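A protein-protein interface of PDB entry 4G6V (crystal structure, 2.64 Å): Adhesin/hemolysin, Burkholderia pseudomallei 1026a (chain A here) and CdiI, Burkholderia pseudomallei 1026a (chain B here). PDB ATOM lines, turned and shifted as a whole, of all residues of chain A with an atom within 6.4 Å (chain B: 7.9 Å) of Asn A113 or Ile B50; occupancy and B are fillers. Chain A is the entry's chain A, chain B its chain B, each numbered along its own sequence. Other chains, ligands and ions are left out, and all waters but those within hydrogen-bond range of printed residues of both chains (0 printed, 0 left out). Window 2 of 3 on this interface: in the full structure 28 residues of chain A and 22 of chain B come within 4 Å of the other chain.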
ATOM      1  N   TYR A 104     -41.359  24.890   3.854  1.00  0.00           N
ATOM      2  CA  TYR A 104     -39.973  24.637   4.237  1.00  0.00           C
ATOM      3  C   TYR A 104     -39.959  23.978   5.614  1.00  0.00           C
ATOM      4  O   TYR A 104     -40.438  24.544   6.607  1.00  0.00           O
ATOM      5  CB  TYR A 104     -39.156  25.934   4.203  1.00  0.00           C
ATOM      6  CG  TYR A 104     -37.844  25.910   4.943  1.00  0.00           C
ATOM      7  CD1 TYR A 104     -36.943  24.856   4.795  1.00  0.00           C
ATOM      8  CD2 TYR A 104     -37.492  26.954   5.778  1.00  0.00           C
ATOM      9  CE1 TYR A 104     -35.735  24.847   5.488  1.00  0.00           C
ATOM     10  CE2 TYR A 104     -36.276  26.963   6.460  1.00  0.00           C
ATOM     11  CZ  TYR A 104     -35.402  25.914   6.316  1.00  0.00           C
ATOM     12  OH  TYR A 104     -34.192  25.954   7.001  1.00  0.00           O
ATOM     13  N   THR A 108     -32.856  20.945  10.743  1.00  0.00           N
ATOM     14  CA  THR A 108     -31.863  21.627  11.550  1.00  0.00           C
ATOM     15  C   THR A 108     -32.561  22.404  12.660  1.00  0.00           C
ATOM     16  O   THR A 108     -33.723  22.837  12.510  1.00  0.00           O
ATOM     17  CB  THR A 108     -31.024  22.623  10.708  1.00  0.00           C
ATOM     18  OG1 THR A 108     -30.082  23.292  11.553  1.00  0.00           O
ATOM     19  CG2 THR A 108     -31.903  23.694  10.056  1.00  0.00           C
ATOM     20  N   ASN A 110     -30.576  24.982  13.924  1.00  0.00           N
ATOM     21  CA  ASN A 110     -29.764  26.197  13.856  1.00  0.00           C
ATOM     22  C   ASN A 110     -30.545  27.367  13.271  1.00  0.00           C
ATOM     23  O   ASN A 110     -30.586  27.560  12.048  1.00  0.00           O
ATOM     24  CB  ASN A 110     -28.514  25.972  13.012  1.00  0.00           C
ATOM     25  CG  ASN A 110     -27.432  27.010  13.283  1.00  0.00           C
ATOM     26  OD1 ASN A 110     -27.534  28.166  12.877  1.00  0.00           O
ATOM     27  ND2 ASN A 110     -26.379  26.590  13.967  1.00  0.00           N
ATOM     28  N   VAL A 111     -31.144  28.157  14.152  1.00  0.00           N
ATOM     29  CA  VAL A 111     -32.009  29.266  13.749  1.00  0.00           C
ATOM     30  C   VAL A 111     -31.389  30.245  12.745  1.00  0.00           C
ATOM     31  O   VAL A 111     -32.053  30.682  11.802  1.00  0.00           O
ATOM     32  CB  VAL A 111     -32.514  30.024  14.986  1.00  0.00           C
ATOM     33  CG1 VAL A 111     -33.068  31.355  14.584  1.00  0.00           C
ATOM     34  CG2 VAL A 111     -33.561  29.170  15.716  1.00  0.00           C
ATOM     35  N   ARG A 112     -30.114  30.572  12.937  1.00  0.00           N
ATOM     36  CA  ARG A 112     -29.424  31.463  12.012  1.00  0.00           C
ATOM     37  C   ARG A 112     -29.391  30.845  10.620  1.00  0.00           C
ATOM     38  O   ARG A 112     -29.703  31.508   9.614  1.00  0.00           O
ATOM     39  CB  ARG A 112     -28.015  31.784  12.517  1.00  0.00           C
ATOM     40  CG  ARG A 112     -28.040  32.539  13.844  1.00  0.00           C
ATOM     41  CD  ARG A 112     -26.648  32.986  14.350  1.00  0.00           C
ATOM     42  NE  ARG A 112     -26.657  33.090  15.817  1.00  0.00           N
ATOM     43  CZ  ARG A 112     -25.564  33.156  16.587  1.00  0.00           C
ATOM     44  NH1 ARG A 112     -24.355  33.142  16.045  1.00  0.00           N
ATOM     45  NH2 ARG A 112     -25.660  33.257  17.909  1.00  0.00           N
ATOM     46  N   ASN A 113     -29.040  29.563  10.580  1.00  0.00           N
ATOM     47  CA  ASN A 113     -28.965  28.818   9.328  1.00  0.00           C
ATOM     48  C   ASN A 113     -30.332  28.715   8.664  1.00  0.00           C
ATOM     49  O   ASN A 113     -30.453  28.811   7.434  1.00  0.00           O
ATOM     50  CB  ASN A 113     -28.348  27.434   9.563  1.00  0.00           C
ATOM     51  CG  ASN A 113     -26.853  27.505   9.886  1.00  0.00           C
ATOM     52  OD1 ASN A 113     -26.313  28.568  10.181  1.00  0.00           O
ATOM     53  ND2 ASN A 113     -26.185  26.368   9.829  1.00  0.00           N
ATOM     54  N   ILE A 114     -31.361  28.542   9.486  1.00  0.00           N
ATOM     55  CA  ILE A 114     -32.715  28.534   8.981  1.00  0.00           C
ATOM     56  C   ILE A 114     -33.012  29.846   8.263  1.00  0.00           C
ATOM     57  O   ILE A 114     -33.552  29.839   7.157  1.00  0.00           O
ATOM     58  CB  ILE A 114     -33.750  28.301  10.103  1.00  0.00           C
ATOM     59  CG1 ILE A 114     -33.483  26.963  10.787  1.00  0.00           C
ATOM     60  CG2 ILE A 114     -35.180  28.369   9.547  1.00  0.00           C
ATOM     61  CD1 ILE A 114     -34.674  26.393  11.505  1.00  0.00           C
ATOM     62  N   ALA A 115     -32.650  30.963   8.889  1.00  0.00           N
ATOM     63  CA  ALA A 115     -32.772  32.268   8.226  1.00  0.00           C
ATOM     64  C   ALA A 115     -31.945  32.318   6.944  1.00  0.00           C
ATOM     65  O   ALA A 115     -32.472  32.701   5.895  1.00  0.00           O
ATOM     66  CB  ALA A 115     -32.383  33.424   9.156  1.00  0.00           C
ATOM     67  N   THR A 116     -30.664  31.935   7.027  1.00  0.00           N
ATOM     68  CA  THR A 116     -29.787  31.966   5.855  1.00  0.00           C
ATOM     69  C   THR A 116     -30.448  31.202   4.707  1.00  0.00           C
ATOM     70  O   THR A 116     -30.373  31.585   3.535  1.00  0.00           O
ATOM     71  CB  THR A 116     -28.391  31.337   6.142  1.00  0.00           C
ATOM     72  OG1 THR A 116     -27.688  32.102   7.132  1.00  0.00           O
ATOM     73  CG2 THR A 116     -27.548  31.288   4.877  1.00  0.00           C
ATOM     74  N   THR A 117     -31.121  30.125   5.071  1.00  0.00           N
ATOM     75  CA  THR A 117     -31.682  29.210   4.099  1.00  0.00           C
ATOM     76  C   THR A 117     -32.860  29.869   3.421  1.00  0.00           C
ATOM     77  O   THR A 117     -32.930  29.928   2.199  1.00  0.00           O
ATOM     78  CB  THR A 117     -32.049  27.852   4.788  1.00  0.00           C
ATOM     79  OG1 THR A 117     -30.838  27.257   5.272  1.00  0.00           O
ATOM     80  CG2 THR A 117     -32.737  26.882   3.833  1.00  0.00           C
ATOM     81  N   ILE A 118     -33.779  30.375   4.229  1.00  0.00           N
ATOM     82  CA  ILE A 118     -34.906  31.137   3.733  1.00  0.00           C
ATOM     83  C   ILE A 118     -34.437  32.270   2.825  1.00  0.00           C
ATOM     84  O   ILE A 118     -34.895  32.403   1.678  1.00  0.00           O
ATOM     85  CB  ILE A 118     -35.679  31.770   4.894  1.00  0.00           C
ATOM     86  CG1 ILE A 118     -36.615  30.742   5.525  1.00  0.00           C
ATOM     87  CG2 ILE A 118     -36.504  32.954   4.394  1.00  0.00           C
ATOM     88  CD1 ILE A 118     -37.040  31.096   6.934  1.00  0.00           C
ATOM     89  N   PHE B   6     -28.754  23.216  -2.176  1.00  0.00           N
ATOM     90  CA  PHE B   6     -27.816  24.297  -1.953  1.00  0.00           C
ATOM     91  C   PHE B   6     -26.444  23.817  -2.381  1.00  0.00           C
ATOM     92  O   PHE B   6     -25.927  22.862  -1.830  1.00  0.00           O
ATOM     93  CB  PHE B   6     -27.784  24.664  -0.481  1.00  0.00           C
ATOM     94  CG  PHE B   6     -28.842  25.617  -0.093  1.00  0.00           C
ATOM     95  CD1 PHE B   6     -28.525  26.841   0.465  1.00  0.00           C
ATOM     96  CD2 PHE B   6     -30.171  25.316  -0.317  1.00  0.00           C
ATOM     97  CE1 PHE B   6     -29.536  27.749   0.807  1.00  0.00           C
ATOM     98  CE2 PHE B   6     -31.188  26.217   0.031  1.00  0.00           C
ATOM     99  CZ  PHE B   6     -30.865  27.429   0.586  1.00  0.00           C
ATOM    100  N   TYR B   8     -22.552  24.649  -2.988  1.00  0.00           N
ATOM    101  CA  TYR B   8     -21.373  25.490  -2.812  1.00  0.00           C
ATOM    102  C   TYR B   8     -20.189  25.002  -3.648  1.00  0.00           C
ATOM    103  O   TYR B   8     -19.926  23.788  -3.742  1.00  0.00           O
ATOM    104  CB  TYR B   8     -20.965  25.523  -1.346  1.00  0.00           C
ATOM    105  CG  TYR B   8     -22.108  25.793  -0.410  1.00  0.00           C
ATOM    106  CD1 TYR B   8     -22.194  26.992   0.264  1.00  0.00           C
ATOM    107  CD2 TYR B   8     -23.113  24.838  -0.206  1.00  0.00           C
ATOM    108  CE1 TYR B   8     -23.240  27.247   1.130  1.00  0.00           C
ATOM    109  CE2 TYR B   8     -24.156  25.077   0.667  1.00  0.00           C
ATOM    110  CZ  TYR B   8     -24.215  26.287   1.331  1.00  0.00           C
ATOM    111  OH  TYR B   8     -25.249  26.552   2.197  1.00  0.00           O
ATOM    112  N   ASP B  44     -21.410  34.919  -0.020  1.00  0.00           N
ATOM    113  CA  ASP B  44     -21.151  35.877   1.048  1.00  0.00           C
ATOM    114  C   ASP B  44     -20.635  35.164   2.304  1.00  0.00           C
ATOM    115  O   ASP B  44     -20.384  33.953   2.292  1.00  0.00           O
ATOM    116  CB  ASP B  44     -22.431  36.621   1.391  1.00  0.00           C
ATOM    117  CG  ASP B  44     -23.477  35.706   1.996  1.00  0.00           C
ATOM    118  OD1 ASP B  44     -23.215  34.479   2.035  1.00  0.00           O
ATOM    119  OD2 ASP B  44     -24.547  36.199   2.436  1.00  0.00           O
ATOM    120  N   PHE B  45     -20.511  35.912   3.397  1.00  0.00           N
ATOM    121  CA  PHE B  45     -19.915  35.374   4.619  1.00  0.00           C
ATOM    122  C   PHE B  45     -20.719  34.216   5.216  1.00  0.00           C
ATOM    123  O   PHE B  45     -20.146  33.280   5.751  1.00  0.00           O
ATOM    124  CB  PHE B  45     -19.713  36.470   5.681  1.00  0.00           C
ATOM    125  CG  PHE B  45     -19.296  35.935   7.016  1.00  0.00           C
ATOM    126  CD1 PHE B  45     -17.954  35.775   7.330  1.00  0.00           C
ATOM    127  CD2 PHE B  45     -20.244  35.540   7.946  1.00  0.00           C
ATOM    128  CE1 PHE B  45     -17.567  35.244   8.560  1.00  0.00           C
ATOM    129  CE2 PHE B  45     -19.869  35.015   9.170  1.00  0.00           C
ATOM    130  CZ  PHE B  45     -18.532  34.865   9.479  1.00  0.00           C
ATOM    131  N   SER B  46     -22.045  34.306   5.132  1.00  0.00           N
ATOM    132  CA  SER B  46     -22.935  33.315   5.725  1.00  0.00           C
ATOM    133  C   SER B  46     -22.816  31.989   5.014  1.00  0.00           C
ATOM    134  O   SER B  46     -22.660  30.971   5.668  1.00  0.00           O
ATOM    135  CB  SER B  46     -24.391  33.785   5.696  1.00  0.00           C
ATOM    136  OG  SER B  46     -24.692  34.601   6.818  1.00  0.00           O
ATOM    137  N   LEU B  47     -22.882  31.998   3.684  1.00  0.00           N
ATOM    138  CA  LEU B  47     -22.721  30.762   2.917  1.00  0.00           C
ATOM    139  C   LEU B  47     -21.327  30.141   3.102  1.00  0.00           C
ATOM    140  O   LEU B  47     -21.189  28.921   3.184  1.00  0.00           O
ATOM    141  CB  LEU B  47     -23.011  30.993   1.435  1.00  0.00           C
ATOM    142  CG  LEU B  47     -24.424  31.470   1.102  1.00  0.00           C
ATOM    143  CD1 LEU B  47     -24.466  32.091  -0.294  1.00  0.00           C
ATOM    144  CD2 LEU B  47     -25.432  30.331   1.232  1.00  0.00           C
ATOM    145  N   LYS B  48     -20.298  30.988   3.166  1.00  0.00           N
ATOM    146  CA  LYS B  48     -18.930  30.533   3.384  1.00  0.00           C
ATOM    147  C   LYS B  48     -18.778  29.843   4.734  1.00  0.00           C
ATOM    148  O   LYS B  48     -17.992  28.900   4.875  1.00  0.00           O
ATOM    149  CB  LYS B  48     -17.931  31.694   3.301  1.00  0.00           C
ATOM    150  CG  LYS B  48     -17.681  32.214   1.896  1.00  0.00           C
ATOM    151  CD  LYS B  48     -16.588  33.267   1.892  1.00  0.00           C
ATOM    152  CE  LYS B  48     -16.376  33.853   0.515  1.00  0.00           C
ATOM    153  NZ  LYS B  48     -15.129  34.670   0.483  1.00  0.00           N
ATOM    154  N   GLU B  49     -19.519  30.335   5.720  1.00  0.00           N
ATOM    155  CA  GLU B  49     -19.477  29.777   7.053  1.00  0.00           C
ATOM    156  C   GLU B  49     -20.035  28.347   7.062  1.00  0.00           C
ATOM    157  O   GLU B  49     -19.399  27.423   7.585  1.00  0.00           O
ATOM    158  CB  GLU B  49     -20.253  30.671   8.013  1.00  0.00           C
ATOM    159  CG  GLU B  49     -20.056  30.335   9.478  1.00  0.00           C
ATOM    160  CD  GLU B  49     -20.883  31.225  10.379  1.00  0.00           C
ATOM    161  OE1 GLU B  49     -21.823  31.877   9.863  1.00  0.00           O
ATOM    162  OE2 GLU B  49     -20.585  31.276  11.594  1.00  0.00           O
ATOM    163  N   ILE B  50     -21.214  28.181   6.466  1.00  0.00           N
ATOM    164  CA  ILE B  50     -21.872  26.879   6.368  1.00  0.00           C
ATOM    165  C   ILE B  50     -21.065  25.890   5.529  1.00  0.00           C
ATOM    166  O   ILE B  50     -20.886  24.751   5.938  1.00  0.00           O
ATOM    167  CB  ILE B  50     -23.310  26.998   5.792  1.00  0.00           C
ATOM    168  CG1 ILE B  50     -24.214  27.831   6.709  1.00  0.00           C
ATOM    169  CG2 ILE B  50     -23.928  25.629   5.582  1.00  0.00           C
ATOM    170  CD1 ILE B  50     -25.633  27.980   6.184  1.00  0.00           C
ATOM    171  N   ALA B  51     -20.553  26.319   4.376  1.00  0.00           N
ATOM    172  CA  ALA B  51     -19.672  25.459   3.570  1.00  0.00           C
ATOM    173  C   ALA B  51     -18.428  24.972   4.332  1.00  0.00           C
ATOM    174  O   ALA B  51     -17.980  23.835   4.142  1.00  0.00           O
ATOM    175  CB  ALA B  51     -19.257  26.149   2.271  1.00  0.00           C
ATOM    176  N   ALA B  52     -17.881  25.829   5.193  1.00  0.00           N
ATOM    177  CA  ALA B  52     -16.640  25.519   5.894  1.00  0.00           C
ATOM    178  C   ALA B  52     -16.841  24.542   7.058  1.00  0.00           C
ATOM    179  O   ALA B  52     -15.897  23.886   7.485  1.00  0.00           O
ATOM    180  CB  ALA B  52     -15.941  26.788   6.363  1.00  0.00           C
ATOM    181  N   GLU B  53     -18.063  24.456   7.564  1.00  0.00           N
ATOM    182  CA  GLU B  53     -18.433  23.434   8.545  1.00  0.00           C
ATOM    183  C   GLU B  53     -18.470  22.035   7.926  1.00  0.00           C
ATOM    184  O   GLU B  53     -18.342  21.038   8.634  1.00  0.00           O
ATOM    185  CB  GLU B  53     -19.800  23.737   9.169  1.00  0.00           C
ATOM    186  CG  GLU B  53     -19.741  24.613  10.407  1.00  0.00           C
ATOM    187  CD  GLU B  53     -21.016  25.416  10.624  1.00  0.00           C
ATOM    188  OE1 GLU B  53     -22.122  24.877  10.378  1.00  0.00           O
ATOM    189  OE2 GLU B  53     -20.919  26.597  11.032  1.00  0.00           O
ATOM    190  N   HIS B  54     -18.640  21.976   6.604  1.00  0.00           N
ATOM    191  CA  HIS B  54     -18.639  20.714   5.866  1.00  0.00           C
ATOM    192  C   HIS B  54     -17.390  20.505   5.020  1.00  0.00           C
ATOM    193  O   HIS B  54     -17.435  19.789   4.018  1.00  0.00           O
ATOM    194  CB  HIS B  54     -19.846  20.653   4.951  1.00  0.00           C
ATOM    195  CG  HIS B  54     -21.140  20.892   5.650  1.00  0.00           C
ATOM    196  ND1 HIS B  54     -21.646  22.151   5.883  1.00  0.00           N
ATOM    197  CD2 HIS B  54     -22.057  20.026   6.167  1.00  0.00           C
ATOM    198  CE1 HIS B  54     -22.810  22.058   6.507  1.00  0.00           C
ATOM    199  NE2 HIS B  54     -23.073  20.770   6.692  1.00  0.00           N
ATOM    200  N   GLY B  55     -16.289  21.147   5.404  1.00  0.00           N
ATOM    201  CA  GLY B  55     -14.999  20.905   4.789  1.00  0.00           C
ATOM    202  C   GLY B  55     -14.543  21.841   3.681  1.00  0.00           C
ATOM    203  O   GLY B  55     -13.359  21.842   3.336  1.00  0.00           O
ATOM    204  N   LEU B  56     -15.460  22.646   3.140  1.00  0.00           N
ATOM    205  CA  LEU B  56     -15.223  23.363   1.886  1.00  0.00           C
ATOM    206  C   LEU B  56     -15.104  24.866   2.049  1.00  0.00           C
ATOM    207  O   LEU B  56     -15.896  25.492   2.753  1.00  0.00           O
ATOM    208  CB  LEU B  56     -16.333  23.047   0.882  1.00  0.00           C
ATOM    209  CG  LEU B  56     -16.278  23.699  -0.495  1.00  0.00           C
ATOM    210  CD1 LEU B  56     -15.577  22.794  -1.461  1.00  0.00           C
ATOM    211  CD2 LEU B  56     -17.658  23.930  -0.980  1.00  0.00           C
ATOM    212  N   ALA B  58     -15.868  27.921   0.135  1.00  0.00           N
ATOM    213  CA  ALA B  58     -16.727  28.281  -1.000  1.00  0.00           C
ATOM    214  C   ALA B  58     -16.431  29.681  -1.531  1.00  0.00           C
ATOM    215  O   ALA B  58     -16.246  30.623  -0.755  1.00  0.00           O
ATOM    216  CB  ALA B  58     -18.216  28.152  -0.624  1.00  0.00           C
ATOM    217  N   LEU B  92     -19.925  21.112  -2.591  1.00  0.00           N
ATOM    218  CA  LEU B  92     -20.697  20.576  -1.479  1.00  0.00           C
ATOM    219  C   LEU B  92     -22.164  20.744  -1.858  1.00  0.00           C
ATOM    220  O   LEU B  92     -22.553  21.809  -2.333  1.00  0.00           O
ATOM    221  CB  LEU B  92     -20.355  21.336  -0.195  1.00  0.00           C
ATOM    222  CG  LEU B  92     -21.355  21.335   0.958  1.00  0.00           C
ATOM    223  CD1 LEU B  92     -21.417  19.973   1.561  1.00  0.00           C
ATOM    224  CD2 LEU B  92     -20.969  22.365   1.999  1.00  0.00           C
ATOM    225  N   LEU B  94     -25.939  20.518  -0.208  1.00  0.00           N
ATOM    226  CA  LEU B  94     -26.842  20.305   0.908  1.00  0.00           C
ATOM    227  C   LEU B  94     -28.319  20.446   0.482  1.00  0.00           C
ATOM    228  O   LEU B  94     -28.796  21.523   0.095  1.00  0.00           O
ATOM    229  CB  LEU B  94     -26.519  21.270   2.051  1.00  0.00           C
ATOM    230  CG  LEU B  94     -25.105  21.315   2.624  1.00  0.00           C
ATOM    231  CD1 LEU B  94     -25.047  22.235   3.820  1.00  0.00           C
ATOM    232  CD2 LEU B  94     -24.643  19.940   3.039  1.00  0.00           C
ATOM    233  N   ASP B  96     -31.813  21.333   0.927  1.00  0.00           N
ATOM    234  CA  ASP B  96     -32.425  22.336   1.797  1.00  0.00           C
ATOM    235  C   ASP B  96     -31.450  22.854   2.841  1.00  0.00           C
ATOM    236  O   ASP B  96     -31.831  23.200   3.972  1.00  0.00           O
ATOM    237  CB  ASP B  96     -33.729  21.813   2.426  1.00  0.00           C
ATOM    238  CG  ASP B  96     -34.899  21.820   1.434  1.00  0.00           C
ATOM    239  OD1 ASP B  96     -34.914  22.704   0.526  1.00  0.00           O
ATOM    240  OD2 ASP B  96     -35.795  20.944   1.560  1.00  0.00           O
ATOM    241  N   ASN B  97     -30.183  22.895   2.437  1.00  0.00           N
ATOM    242  CA  ASN B  97     -29.131  23.504   3.233  1.00  0.00           C
ATOM    243  C   ASN B  97     -28.956  22.788   4.565  1.00  0.00           C
ATOM    244  O   ASN B  97     -28.482  23.373   5.535  1.00  0.00           O
ATOM    245  CB  ASN B  97     -29.430  25.001   3.436  1.00  0.00           C
ATOM    246  CG  ASN B  97     -28.165  25.857   3.474  1.00  0.00           C
ATOM    247  OD1 ASN B  97     -27.111  25.473   2.949  1.00  0.00           O
ATOM    248  ND2 ASN B  97     -28.266  27.018   4.111  1.00  0.00           N
ATOM    249  N   GLU B  98     -29.336  21.512   4.591  1.00  0.00           N
ATOM    250  CA  GLU B  98     -29.293  20.691   5.810  1.00  0.00           C
ATOM    251  C   GLU B  98     -28.602  19.355   5.617  1.00  0.00           C
ATOM    252  O   GLU B  98     -27.709  19.006   6.379  1.00  0.00           O
ATOM    253  CB  GLU B  98     -30.704  20.417   6.343  1.00  0.00           C
ATOM    254  CG  GLU B  98     -31.344  21.626   6.966  1.00  0.00           C
ATOM    255  CD  GLU B  98     -32.742  21.372   7.468  1.00  0.00           C
ATOM    256  OE1 GLU B  98     -33.443  22.370   7.714  1.00  0.00           O
ATOM    257  OE2 GLU B  98     -33.145  20.202   7.613  1.00  0.00           O
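The side-chain hydroxyl (OG1) of Thr A108 sits at hydrogen-bond distance from the backbone NH (N) of Asn A110 (3.0 Å).
The side-chain amide oxygen (OD1) of Asn A110 sits close to the side-chain amide oxygen (OD1) of Asn A113 (3.0 Å).
OG1 of Thr A116 lies within hydrogen-bond range of O of Arg A112, at 3.3 Å.
The backbone carbonyl oxygen of Asn A113 is in hydrogen-bond range of the side-chain hydroxyl of Thr A117.
The backbone NH (N) of Ser B46 sits close to the side-chain carboxylate (OD1) of Asp B44 (3.3 Å).
The backbone carbonyl oxygen (O) of Ile B50 lies within hydrogen-bond range of a ring nitrogen (ND1) of His B54, 2.7 Å away.
Of chain B, only Ile B50 (3.9 Å) comes within 4 Å of Asn A113.
Of the printed residues of chain A, Phe B6 touches Thr A117 (3.6 Å).
Ile B50 touches just one residue of chain A: Asn A113 (3.9 Å).
Of the printed residues of chain A, Asn B97 touches Thr A117.
The nearest residue of chain A that does not touch Ile B50 is Thr A116 (4.04 Å).
Of the 21 printed residues of chain B, 6 touch a printed residue of chain A.
Printed residues of chain A that touch a printed residue of chain B: Tyr A104, Thr A108, Asn A113, Thr A116 and Thr A117.
Hydrophobic or aromatic side chains of chain A that line the printed part of chain B: Tyr A104.
Among the printed residues, 7 pairs touch across the chains.
N of Thr A108 lies within hydrogen-bond range of OE2 of Glu B98, 3.2 Å away.
ND2 of Asn B97 lies within hydrogen-bond range of OG1 of Thr A117, at 2.8 Å.
Tyr A104 touches Glu B98.
Asn A113 touches Ile B50 (CG to CD1, 3.9 Å).
Thr A116 touches Ser B46.
Thr A117 touches Phe B6 (O to CZ, 3.6 Å).
CG2 of Thr A117 touches O of Asp B96, 3.8 Å away.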
